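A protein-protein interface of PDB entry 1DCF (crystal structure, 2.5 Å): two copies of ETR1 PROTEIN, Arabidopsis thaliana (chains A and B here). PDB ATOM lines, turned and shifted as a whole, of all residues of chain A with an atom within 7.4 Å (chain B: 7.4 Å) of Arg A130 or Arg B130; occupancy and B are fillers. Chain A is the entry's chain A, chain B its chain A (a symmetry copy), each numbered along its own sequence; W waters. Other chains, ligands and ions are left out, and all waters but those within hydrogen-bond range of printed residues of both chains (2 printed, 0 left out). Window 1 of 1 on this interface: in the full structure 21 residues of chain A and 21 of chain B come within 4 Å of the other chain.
O of Asp A107 sits at hydrogen-bond distance from N of Leu B132, at 2.9 Å.
NH1 of Arg B130 lies close to NH1 of Arg A130 (2.6 Å).
N of Leu A132 is in hydrogen-bond range of O of Asp B107 (2.9 Å).
SD of Met A102 sits close to O of Pro B129.
The side-chain sulfur (SD) of Met B102 lies close to the backbone carbonyl oxygen (O) of Pro A129, 3.8 Å away.
The backbone NH (N) of Leu A106 lies within hydrogen-bond range of the backbone carbonyl oxygen (O) of Cys A101 (2.7 Å).
The backbone carbonyl oxygen (O) of Cys B101 sits at hydrogen-bond distance from the backbone NH (N) of Leu B106.
CG2 of Val B131 touches CB of Cys A101 (3.8 Å).
Met A102 touches Val B131.
Leu B132 touches Gly A108 (O to CA, 3.1 Å).
CD1 of Leu B132 touches CB of Asp A125 (3.5 Å).
CD2 of Leu A126 touches CD1 of Leu B132 (3.3 Å).
Val A131 touches Met B102.
O of Leu A132 touches CA of Gly B108 (3.1 Å).
Asp B125 touches Leu A132.
CD1 of Leu A132 touches CD2 of Leu B126, at 3.3 Å.
NH2 of Arg B130 touches CD2 of Leu A132, at 3.1 Å.
Arg B130 touches just these residues of chain A: Arg A130 and Leu A132.
Of the printed residues of chain B, Pro A129 touches Met B102 (3.8 Å).
Printed residues of chain B within 4 Å of Cys A101: Val B131.
Of the printed residues of chain A, Asp B125 touches Leu A132 (3.5 Å).
Printed residues of chain A within 4 Å of Cys B101: Val A131.
Of the 18 printed residues of chain B, 11 touch a printed residue of chain A.
Of the 18 printed residues of chain A, 11 touch a printed residue of chain B.
Along chain A the printed residues that touch a printed residue of chain B span positions 101 to 132.
Among the printed residues, no Asp or Glu carboxylate lies within 4 Å of a Lys or Arg side-chain nitrogen of the other chain.
Cys A101 touches Val B131, and with the chains exchanged Val A131 touches Cys B101.
Asp A107 touches Val B131, and with the chains exchanged Val A131 touches Asp B107.
Asp A125 touches Leu B132, and with the chains exchanged Leu A132 touches Asp B125.
Arg B130 touches its own counterpart, Arg A130.
18 positions are printed for both chains.
Water W2 lies within hydrogen-bond range of the guanidinium group (NH1) of Arg B130 (2.8 Å) and the guanidinium group (NE) of Arg A130 (3.5 Å).
Water W1 lies within hydrogen-bond range of the guanidinium group of Arg A130 (2.8 Å) and the guanidinium group of Arg B130 (3.5 Å).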
ATOM      1  N   LYS A  98       7.352 -10.216 -12.422  1.00  0.00           N
ATOM      2  CA  LYS A  98       6.458 -11.161 -11.747  1.00  0.00           C
ATOM      3  C   LYS A  98       5.858 -10.607 -10.453  1.00  0.00           C
ATOM      4  O   LYS A  98       4.646 -10.698 -10.233  1.00  0.00           O
ATOM      5  CB  LYS A  98       7.194 -12.473 -11.467  1.00  0.00           C
ATOM      6  N   CYS A 101       3.163  -7.982 -11.334  1.00  0.00           N
ATOM      7  CA  CYS A 101       1.941  -8.552 -11.874  1.00  0.00           C
ATOM      8  C   CYS A 101       1.046  -9.134 -10.786  1.00  0.00           C
ATOM      9  O   CYS A 101      -0.177  -8.952 -10.812  1.00  0.00           O
ATOM     10  CB  CYS A 101       2.276  -9.636 -12.898  1.00  0.00           C
ATOM     11  SG  CYS A 101       3.080  -9.013 -14.387  1.00  0.00           S
ATOM     12  N   MET A 102       1.652  -9.829  -9.825  1.00  0.00           N
ATOM     13  CA  MET A 102       0.887 -10.454  -8.755  1.00  0.00           C
ATOM     14  C   MET A 102       0.178  -9.460  -7.885  1.00  0.00           C
ATOM     15  O   MET A 102      -1.040  -9.528  -7.719  1.00  0.00           O
ATOM     16  CB  MET A 102       1.773 -11.326  -7.873  1.00  0.00           C
ATOM     17  CG  MET A 102       2.309 -12.549  -8.571  1.00  0.00           C
ATOM     18  SD  MET A 102       3.135 -13.640  -7.433  1.00  0.00           S
ATOM     19  CE  MET A 102       3.628 -14.947  -8.560  1.00  0.00           C
ATOM     20  N   GLY A 105      -2.576  -7.741  -9.830  1.00  0.00           N
ATOM     21  CA  GLY A 105      -3.646  -8.468 -10.477  1.00  0.00           C
ATOM     22  C   GLY A 105      -3.501  -8.971 -11.890  1.00  0.00           C
ATOM     23  O   GLY A 105      -4.500  -9.444 -12.439  1.00  0.00           O
ATOM     24  N   LEU A 106      -2.313  -8.865 -12.496  1.00  0.00           N
ATOM     25  CA  LEU A 106      -2.122  -9.386 -13.855  1.00  0.00           C
ATOM     26  C   LEU A 106      -2.124 -10.900 -13.729  1.00  0.00           C
ATOM     27  O   LEU A 106      -1.481 -11.456 -12.835  1.00  0.00           O
ATOM     28  CB  LEU A 106      -0.786  -8.941 -14.470  1.00  0.00           C
ATOM     29  CG  LEU A 106      -0.595  -7.505 -14.981  1.00  0.00           C
ATOM     30  CD1 LEU A 106      -1.380  -7.292 -16.260  1.00  0.00           C
ATOM     31  CD2 LEU A 106      -1.015  -6.514 -13.909  1.00  0.00           C
ATOM     32  N   ASP A 107      -2.845 -11.564 -14.623  1.00  0.00           N
ATOM     33  CA  ASP A 107      -2.934 -13.019 -14.610  1.00  0.00           C
ATOM     34  C   ASP A 107      -1.823 -13.686 -15.419  1.00  0.00           C
ATOM     35  O   ASP A 107      -1.497 -14.851 -15.193  1.00  0.00           O
ATOM     36  CB  ASP A 107      -4.283 -13.441 -15.166  1.00  0.00           C
ATOM     37  CG  ASP A 107      -5.421 -12.752 -14.472  1.00  0.00           C
ATOM     38  OD1 ASP A 107      -5.648 -13.034 -13.279  1.00  0.00           O
ATOM     39  OD2 ASP A 107      -6.079 -11.911 -15.120  1.00  0.00           O
ATOM     40  N   GLY A 108      -1.245 -12.955 -16.365  1.00  0.00           N
ATOM     41  CA  GLY A 108      -0.194 -13.536 -17.174  1.00  0.00           C
ATOM     42  C   GLY A 108       0.734 -12.465 -17.674  1.00  0.00           C
ATOM     43  O   GLY A 108       0.437 -11.287 -17.533  1.00  0.00           O
ATOM     44  N   VAL A 122       0.225 -18.598 -23.547  1.00  0.00           N
ATOM     45  CA  VAL A 122      -0.445 -17.855 -22.493  1.00  0.00           C
ATOM     46  C   VAL A 122      -1.959 -17.932 -22.618  1.00  0.00           C
ATOM     47  O   VAL A 122      -2.639 -18.327 -21.673  1.00  0.00           O
ATOM     48  CB  VAL A 122       0.014 -16.391 -22.484  1.00  0.00           C
ATOM     49  CG1 VAL A 122      -0.743 -15.602 -21.431  1.00  0.00           C
ATOM     50  CG2 VAL A 122       1.501 -16.340 -22.179  1.00  0.00           C
ATOM     51  N   SER A 124      -3.650 -20.056 -24.055  1.00  0.00           N
ATOM     52  CA  SER A 124      -4.046 -21.436 -23.810  1.00  0.00           C
ATOM     53  C   SER A 124      -4.105 -21.705 -22.310  1.00  0.00           C
ATOM     54  O   SER A 124      -5.124 -22.173 -21.792  1.00  0.00           O
ATOM     55  CB  SER A 124      -3.074 -22.407 -24.482  1.00  0.00           C
ATOM     56  OG  SER A 124      -3.126 -22.274 -25.895  1.00  0.00           O
ATOM     57  N   ASP A 125      -3.022 -21.397 -21.606  1.00  0.00           N
ATOM     58  CA  ASP A 125      -2.995 -21.617 -20.174  1.00  0.00           C
ATOM     59  C   ASP A 125      -4.115 -20.864 -19.486  1.00  0.00           C
ATOM     60  O   ASP A 125      -4.908 -21.446 -18.744  1.00  0.00           O
ATOM     61  CB  ASP A 125      -1.649 -21.192 -19.607  1.00  0.00           C
ATOM     62  CG  ASP A 125      -0.529 -22.097 -20.055  1.00  0.00           C
ATOM     63  OD1 ASP A 125       0.644 -21.803 -19.745  1.00  0.00           O
ATOM     64  OD2 ASP A 125      -0.827 -23.115 -20.714  1.00  0.00           O
ATOM     65  N   LEU A 126      -4.186 -19.566 -19.742  1.00  0.00           N
ATOM     66  CA  LEU A 126      -5.211 -18.729 -19.136  1.00  0.00           C
ATOM     67  C   LEU A 126      -6.617 -19.229 -19.422  1.00  0.00           C
ATOM     68  O   LEU A 126      -7.437 -19.338 -18.516  1.00  0.00           O
ATOM     69  CB  LEU A 126      -5.087 -17.302 -19.651  1.00  0.00           C
ATOM     70  CG  LEU A 126      -3.756 -16.605 -19.411  1.00  0.00           C
ATOM     71  CD1 LEU A 126      -3.803 -15.225 -20.032  1.00  0.00           C
ATOM     72  CD2 LEU A 126      -3.487 -16.514 -17.925  1.00  0.00           C
ATOM     73  N   LEU A 127      -6.885 -19.533 -20.687  1.00  0.00           N
ATOM     74  CA  LEU A 127      -8.203 -19.985 -21.115  1.00  0.00           C
ATOM     75  C   LEU A 127      -8.556 -21.444 -20.845  1.00  0.00           C
ATOM     76  O   LEU A 127      -9.730 -21.776 -20.681  1.00  0.00           O
ATOM     77  CB  LEU A 127      -8.368 -19.715 -22.604  1.00  0.00           C
ATOM     78  CG  LEU A 127      -8.222 -18.256 -23.033  1.00  0.00           C
ATOM     79  CD1 LEU A 127      -8.304 -18.170 -24.552  1.00  0.00           C
ATOM     80  CD2 LEU A 127      -9.303 -17.408 -22.368  1.00  0.00           C
ATOM     81  N   GLU A 128      -7.560 -22.321 -20.810  1.00  0.00           N
ATOM     82  CA  GLU A 128      -7.847 -23.725 -20.575  1.00  0.00           C
ATOM     83  C   GLU A 128      -8.094 -24.080 -19.119  1.00  0.00           C
ATOM     84  O   GLU A 128      -7.528 -23.466 -18.206  1.00  0.00           O
ATOM     85  CB  GLU A 128      -6.732 -24.600 -21.144  1.00  0.00           C
ATOM     86  CG  GLU A 128      -6.711 -24.617 -22.661  1.00  0.00           C
ATOM     87  CD  GLU A 128      -5.583 -25.456 -23.227  1.00  0.00           C
ATOM     88  OE1 GLU A 128      -5.500 -25.567 -24.467  1.00  0.00           O
ATOM     89  OE2 GLU A 128      -4.781 -25.999 -22.439  1.00  0.00           O
ATOM     90  N   PRO A 129      -8.961 -25.081 -18.888  1.00  0.00           N
ATOM     91  CA  PRO A 129      -9.349 -25.590 -17.570  1.00  0.00           C
ATOM     92  C   PRO A 129      -8.173 -26.087 -16.744  1.00  0.00           C
ATOM     93  O   PRO A 129      -7.343 -26.871 -17.218  1.00  0.00           O
ATOM     94  CB  PRO A 129     -10.324 -26.715 -17.920  1.00  0.00           C
ATOM     95  CG  PRO A 129     -10.954 -26.199 -19.202  1.00  0.00           C
ATOM     96  CD  PRO A 129      -9.682 -25.832 -19.930  1.00  0.00           C
ATOM     97  N   ARG A 130      -8.110 -25.608 -15.506  1.00  0.00           N
ATOM     98  CA  ARG A 130      -7.073 -25.997 -14.561  1.00  0.00           C
ATOM     99  C   ARG A 130      -7.736 -26.341 -13.227  1.00  0.00           C
ATOM    100  O   ARG A 130      -8.692 -25.694 -12.796  1.00  0.00           O
ATOM    101  CB  ARG A 130      -6.062 -24.862 -14.360  1.00  0.00           C
ATOM    102  CG  ARG A 130      -4.957 -25.204 -13.367  1.00  0.00           C
ATOM    103  CD  ARG A 130      -3.998 -24.042 -13.139  1.00  0.00           C
ATOM    104  NE  ARG A 130      -3.350 -23.597 -14.370  1.00  0.00           N
ATOM    105  CZ  ARG A 130      -2.344 -22.728 -14.412  1.00  0.00           C
ATOM    106  NH1 ARG A 130      -1.863 -22.204 -13.291  1.00  0.00           N
ATOM    107  NH2 ARG A 130      -1.822 -22.375 -15.578  1.00  0.00           N
ATOM    108  N   VAL A 131      -7.224 -27.380 -12.584  1.00  0.00           N
ATOM    109  CA  VAL A 131      -7.746 -27.827 -11.304  1.00  0.00           C
ATOM    110  C   VAL A 131      -6.559 -28.149 -10.436  1.00  0.00           C
ATOM    111  O   VAL A 131      -5.677 -28.910 -10.839  1.00  0.00           O
ATOM    112  CB  VAL A 131      -8.620 -29.081 -11.479  1.00  0.00           C
ATOM    113  CG1 VAL A 131      -8.992 -29.668 -10.125  1.00  0.00           C
ATOM    114  CG2 VAL A 131      -9.875 -28.714 -12.255  1.00  0.00           C
ATOM    115  N   LEU A 132      -6.530 -27.546  -9.250  1.00  0.00           N
ATOM    116  CA  LEU A 132      -5.444 -27.776  -8.313  1.00  0.00           C
ATOM    117  C   LEU A 132      -5.806 -28.978  -7.468  1.00  0.00           C
ATOM    118  O   LEU A 132      -6.616 -28.888  -6.547  1.00  0.00           O
ATOM    119  CB  LEU A 132      -5.251 -26.549  -7.421  1.00  0.00           C
ATOM    120  CG  LEU A 132      -5.001 -25.252  -8.186  1.00  0.00           C
ATOM    121  CD1 LEU A 132      -4.868 -24.082  -7.214  1.00  0.00           C
ATOM    122  CD2 LEU A 132      -3.746 -25.402  -9.027  1.00  0.00           C
ATOM    123  N   TYR A 133      -5.230 -30.123  -7.820  1.00  0.00           N
ATOM    124  CA  TYR A 133      -5.480 -31.344  -7.077  1.00  0.00           C
ATOM    125  C   TYR A 133      -4.548 -31.358  -5.895  1.00  0.00           C
ATOM    126  O   TYR A 133      -3.713 -30.472  -5.791  1.00  0.00           O
ATOM    127  N   LYS B  98     -10.291 -35.663 -11.778  1.00  0.00           N
ATOM    128  CA  LYS B  98      -9.760 -34.466 -12.435  1.00  0.00           C
ATOM    129  C   LYS B  98     -10.570 -34.041 -13.663  1.00  0.00           C
ATOM    130  O   LYS B  98     -10.920 -32.865 -13.808  1.00  0.00           O
ATOM    131  CB  LYS B  98      -8.295 -34.683 -12.820  1.00  0.00           C
ATOM    132  N   CYS B 101     -13.905 -32.477 -12.495  1.00  0.00           N
ATOM    133  CA  CYS B 101     -13.762 -31.159 -11.903  1.00  0.00           C
ATOM    134  C   CYS B 101     -13.597 -30.069 -12.956  1.00  0.00           C
ATOM    135  O   CYS B 101     -14.190 -28.989 -12.843  1.00  0.00           O
ATOM    136  CB  CYS B 101     -12.565 -31.139 -10.952  1.00  0.00           C
ATOM    137  SG  CYS B 101     -12.773 -32.174  -9.492  1.00  0.00           S
ATOM    138  N   MET B 102     -12.798 -30.350 -13.984  1.00  0.00           N
ATOM    139  CA  MET B 102     -12.548 -29.368 -15.030  1.00  0.00           C
ATOM    140  C   MET B 102     -13.779 -29.013 -15.807  1.00  0.00           C
ATOM    141  O   MET B 102     -14.149 -27.843 -15.898  1.00  0.00           O
ATOM    142  CB  MET B 102     -11.480 -29.852 -16.005  1.00  0.00           C
ATOM    143  CG  MET B 102     -10.105 -29.956 -15.397  1.00  0.00           C
ATOM    144  SD  MET B 102      -8.871 -30.297 -16.634  1.00  0.00           S
ATOM    145  CE  MET B 102      -7.405 -30.350 -15.600  1.00  0.00           C
ATOM    146  N   GLY B 105     -16.219 -27.126 -13.615  1.00  0.00           N
ATOM    147  CA  GLY B 105     -15.869 -25.899 -12.934  1.00  0.00           C
ATOM    148  C   GLY B 105     -15.257 -25.921 -11.556  1.00  0.00           C
ATOM    149  O   GLY B 105     -15.126 -24.845 -10.966  1.00  0.00           O
ATOM    150  N   LEU B 106     -14.905 -27.097 -11.024  1.00  0.00           N
ATOM    151  CA  LEU B 106     -14.264 -27.154  -9.705  1.00  0.00           C
ATOM    152  C   LEU B 106     -12.856 -26.616  -9.898  1.00  0.00           C
ATOM    153  O   LEU B 106     -12.171 -26.983 -10.855  1.00  0.00           O
ATOM    154  CB  LEU B 106     -14.178 -28.586  -9.157  1.00  0.00           C
ATOM    155  CG  LEU B 106     -15.422 -29.292  -8.597  1.00  0.00           C
ATOM    156  CD1 LEU B 106     -15.812 -28.688  -7.262  1.00  0.00           C
ATOM    157  CD2 LEU B 106     -16.563 -29.197  -9.594  1.00  0.00           C
ATOM    158  N   ASP B 107     -12.428 -25.748  -8.989  1.00  0.00           N
ATOM    159  CA  ASP B 107     -11.098 -25.155  -9.062  1.00  0.00           C
ATOM    160  C   ASP B 107     -10.037 -25.997  -8.356  1.00  0.00           C
ATOM    161  O   ASP B 107      -8.848 -25.884  -8.655  1.00  0.00           O
ATOM    162  CB  ASP B 107     -11.137 -23.770  -8.440  1.00  0.00           C
ATOM    163  CG  ASP B 107     -12.220 -22.915  -9.028  1.00  0.00           C
ATOM    164  OD1 ASP B 107     -12.112 -22.552 -10.215  1.00  0.00           O
ATOM    165  OD2 ASP B 107     -13.194 -22.623  -8.303  1.00  0.00           O
ATOM    166  N   GLY B 108     -10.460 -26.836  -7.418  1.00  0.00           N
ATOM    167  CA  GLY B 108      -9.500 -27.652  -6.704  1.00  0.00           C
ATOM    168  C   GLY B 108     -10.147 -28.918  -6.218  1.00  0.00           C
ATOM    169  O   GLY B 108     -11.361 -29.045  -6.287  1.00  0.00           O
ATOM    170  N   VAL B 122      -4.210 -26.554  -0.603  1.00  0.00           N
ATOM    171  CA  VAL B 122      -5.204 -26.141  -1.578  1.00  0.00           C
ATOM    172  C   VAL B 122      -5.650 -24.703  -1.360  1.00  0.00           C
ATOM    173  O   VAL B 122      -5.577 -23.886  -2.276  1.00  0.00           O
ATOM    174  CB  VAL B 122      -6.416 -27.084  -1.551  1.00  0.00           C
ATOM    175  CG1 VAL B 122      -7.484 -26.604  -2.518  1.00  0.00           C
ATOM    176  CG2 VAL B 122      -5.967 -28.479  -1.948  1.00  0.00           C
ATOM    177  N   SER B 124      -4.158 -22.442   0.087  1.00  0.00           N
ATOM    178  CA  SER B 124      -3.019 -21.577  -0.193  1.00  0.00           C
ATOM    179  C   SER B 124      -2.884 -21.361  -1.697  1.00  0.00           C
ATOM    180  O   SER B 124      -2.834 -20.221  -2.169  1.00  0.00           O
ATOM    181  CB  SER B 124      -1.731 -22.176   0.371  1.00  0.00           C
ATOM    182  OG  SER B 124      -1.782 -22.237   1.789  1.00  0.00           O
ATOM    183  N   ASP B 125      -2.842 -22.451  -2.454  1.00  0.00           N
ATOM    184  CA  ASP B 125      -2.719 -22.335  -3.893  1.00  0.00           C
ATOM    185  C   ASP B 125      -3.856 -21.520  -4.475  1.00  0.00           C
ATOM    186  O   ASP B 125      -3.635 -20.541  -5.189  1.00  0.00           O
ATOM    187  CB  ASP B 125      -2.686 -23.718  -4.527  1.00  0.00           C
ATOM    188  CG  ASP B 125      -1.421 -24.468  -4.191  1.00  0.00           C
ATOM    189  OD1 ASP B 125      -1.309 -25.655  -4.563  1.00  0.00           O
ATOM    190  OD2 ASP B 125      -0.529 -23.863  -3.561  1.00  0.00           O
ATOM    191  N   LEU B 126      -5.079 -21.919  -4.157  1.00  0.00           N
ATOM    192  CA  LEU B 126      -6.256 -21.227  -4.657  1.00  0.00           C
ATOM    193  C   LEU B 126      -6.259 -19.749  -4.305  1.00  0.00           C
ATOM    194  O   LEU B 126      -6.499 -18.903  -5.161  1.00  0.00           O
ATOM    195  CB  LEU B 126      -7.516 -21.865  -4.089  1.00  0.00           C
ATOM    196  CG  LEU B 126      -7.721 -23.344  -4.383  1.00  0.00           C
ATOM    197  CD1 LEU B 126      -8.989 -23.811  -3.699  1.00  0.00           C
ATOM    198  CD2 LEU B 126      -7.808 -23.562  -5.877  1.00  0.00           C
ATOM    199  N   LEU B 127      -5.986 -19.448  -3.040  1.00  0.00           N
ATOM    200  CA  LEU B 127      -5.993 -18.076  -2.549  1.00  0.00           C
ATOM    201  C   LEU B 127      -4.768 -17.223  -2.861  1.00  0.00           C
ATOM    202  O   LEU B 127      -4.875 -16.001  -2.964  1.00  0.00           O
ATOM    203  CB  LEU B 127      -6.208 -18.082  -1.042  1.00  0.00           C
ATOM    204  CG  LEU B 127      -7.494 -18.749  -0.559  1.00  0.00           C
ATOM    205  CD1 LEU B 127      -7.506 -18.770   0.965  1.00  0.00           C
ATOM    206  CD2 LEU B 127      -8.705 -18.005  -1.115  1.00  0.00           C
ATOM    207  N   GLU B 128      -3.604 -17.845  -2.998  1.00  0.00           N
ATOM    208  CA  GLU B 128      -2.405 -17.075  -3.276  1.00  0.00           C
ATOM    209  C   GLU B 128      -2.252 -16.655  -4.728  1.00  0.00           C
ATOM    210  O   GLU B 128      -2.688 -17.358  -5.647  1.00  0.00           O
ATOM    211  CB  GLU B 128      -1.163 -17.837  -2.820  1.00  0.00           C
ATOM    212  CG  GLU B 128      -1.042 -17.918  -1.310  1.00  0.00           C
ATOM    213  CD  GLU B 128       0.171 -18.705  -0.855  1.00  0.00           C
ATOM    214  OE1 GLU B 128       0.383 -18.799   0.371  1.00  0.00           O
ATOM    215  OE2 GLU B 128       0.906 -19.230  -1.716  1.00  0.00           O
ATOM    216  N   PRO B 129      -1.631 -15.483  -4.947  1.00  0.00           N
ATOM    217  CA  PRO B 129      -1.374 -14.883  -6.259  1.00  0.00           C
ATOM    218  C   PRO B 129      -0.554 -15.772  -7.181  1.00  0.00           C
ATOM    219  O   PRO B 129       0.498 -16.296  -6.796  1.00  0.00           O
ATOM    220  CB  PRO B 129      -0.638 -13.592  -5.898  1.00  0.00           C
ATOM    221  CG  PRO B 129      -1.257 -13.240  -4.556  1.00  0.00           C
ATOM    222  CD  PRO B 129      -1.112 -14.591  -3.896  1.00  0.00           C
ATOM    223  N   ARG B 130      -1.060 -15.944  -8.397  1.00  0.00           N
ATOM    224  CA  ARG B 130      -0.397 -16.736  -9.423  1.00  0.00           C
ATOM    225  C   ARG B 130      -0.390 -15.936 -10.726  1.00  0.00           C
ATOM    226  O   ARG B 130      -1.355 -15.248 -11.066  1.00  0.00           O
ATOM    227  CB  ARG B 130      -1.120 -18.070  -9.638  1.00  0.00           C
ATOM    228  CG  ARG B 130      -0.480 -18.940 -10.714  1.00  0.00           C
ATOM    229  CD  ARG B 130      -1.249 -20.234 -10.951  1.00  0.00           C
ATOM    230  NE  ARG B 130      -1.361 -21.050  -9.746  1.00  0.00           N
ATOM    231  CZ  ARG B 130      -1.823 -22.298  -9.730  1.00  0.00           C
ATOM    232  NH1 ARG B 130      -2.218 -22.881 -10.855  1.00  0.00           N
ATOM    233  NH2 ARG B 130      -1.896 -22.962  -8.585  1.00  0.00           N
ATOM    234  N   VAL B 131       0.719 -16.022 -11.446  1.00  0.00           N
ATOM    235  CA  VAL B 131       0.873 -15.320 -12.708  1.00  0.00           C
ATOM    236  C   VAL B 131       1.531 -16.279 -13.664  1.00  0.00           C
ATOM    237  O   VAL B 131       2.576 -16.855 -13.353  1.00  0.00           O
ATOM    238  CB  VAL B 131       1.754 -14.071 -12.534  1.00  0.00           C
ATOM    239  CG1 VAL B 131       2.088 -13.457 -13.886  1.00  0.00           C
ATOM    240  CG2 VAL B 131       1.026 -13.060 -11.664  1.00  0.00           C
ATOM    241  N   LEU B 132       0.901 -16.465 -14.822  1.00  0.00           N
ATOM    242  CA  LEU B 132       1.433 -17.358 -15.835  1.00  0.00           C
ATOM    243  C   LEU B 132       2.378 -16.561 -16.709  1.00  0.00           C
ATOM    244  O   LEU B 132       1.953 -15.794 -17.571  1.00  0.00           O
ATOM    245  CB  LEU B 132       0.295 -17.929 -16.682  1.00  0.00           C
ATOM    246  CG  LEU B 132      -0.783 -18.651 -15.879  1.00  0.00           C
ATOM    247  CD1 LEU B 132      -1.894 -19.142 -16.804  1.00  0.00           C
ATOM    248  CD2 LEU B 132      -0.153 -19.810 -15.127  1.00  0.00           C
ATOM    249  N   TYR B 133       3.671 -16.714 -16.446  1.00  0.00           N
ATOM    250  CA  TYR B 133       4.679 -16.020 -17.225  1.00  0.00           C
ATOM    251  C   TYR B 133       4.940 -16.834 -18.463  1.00  0.00           C
ATOM    252  O   TYR B 133       4.395 -17.921 -18.581  1.00  0.00           O
HETATM  253  O   HOH W   1       0.702 -21.529 -12.502  1.00  0.00           O
HETATM  254  O   HOH W   2      -2.010 -25.483 -11.776  1.00  0.00           O
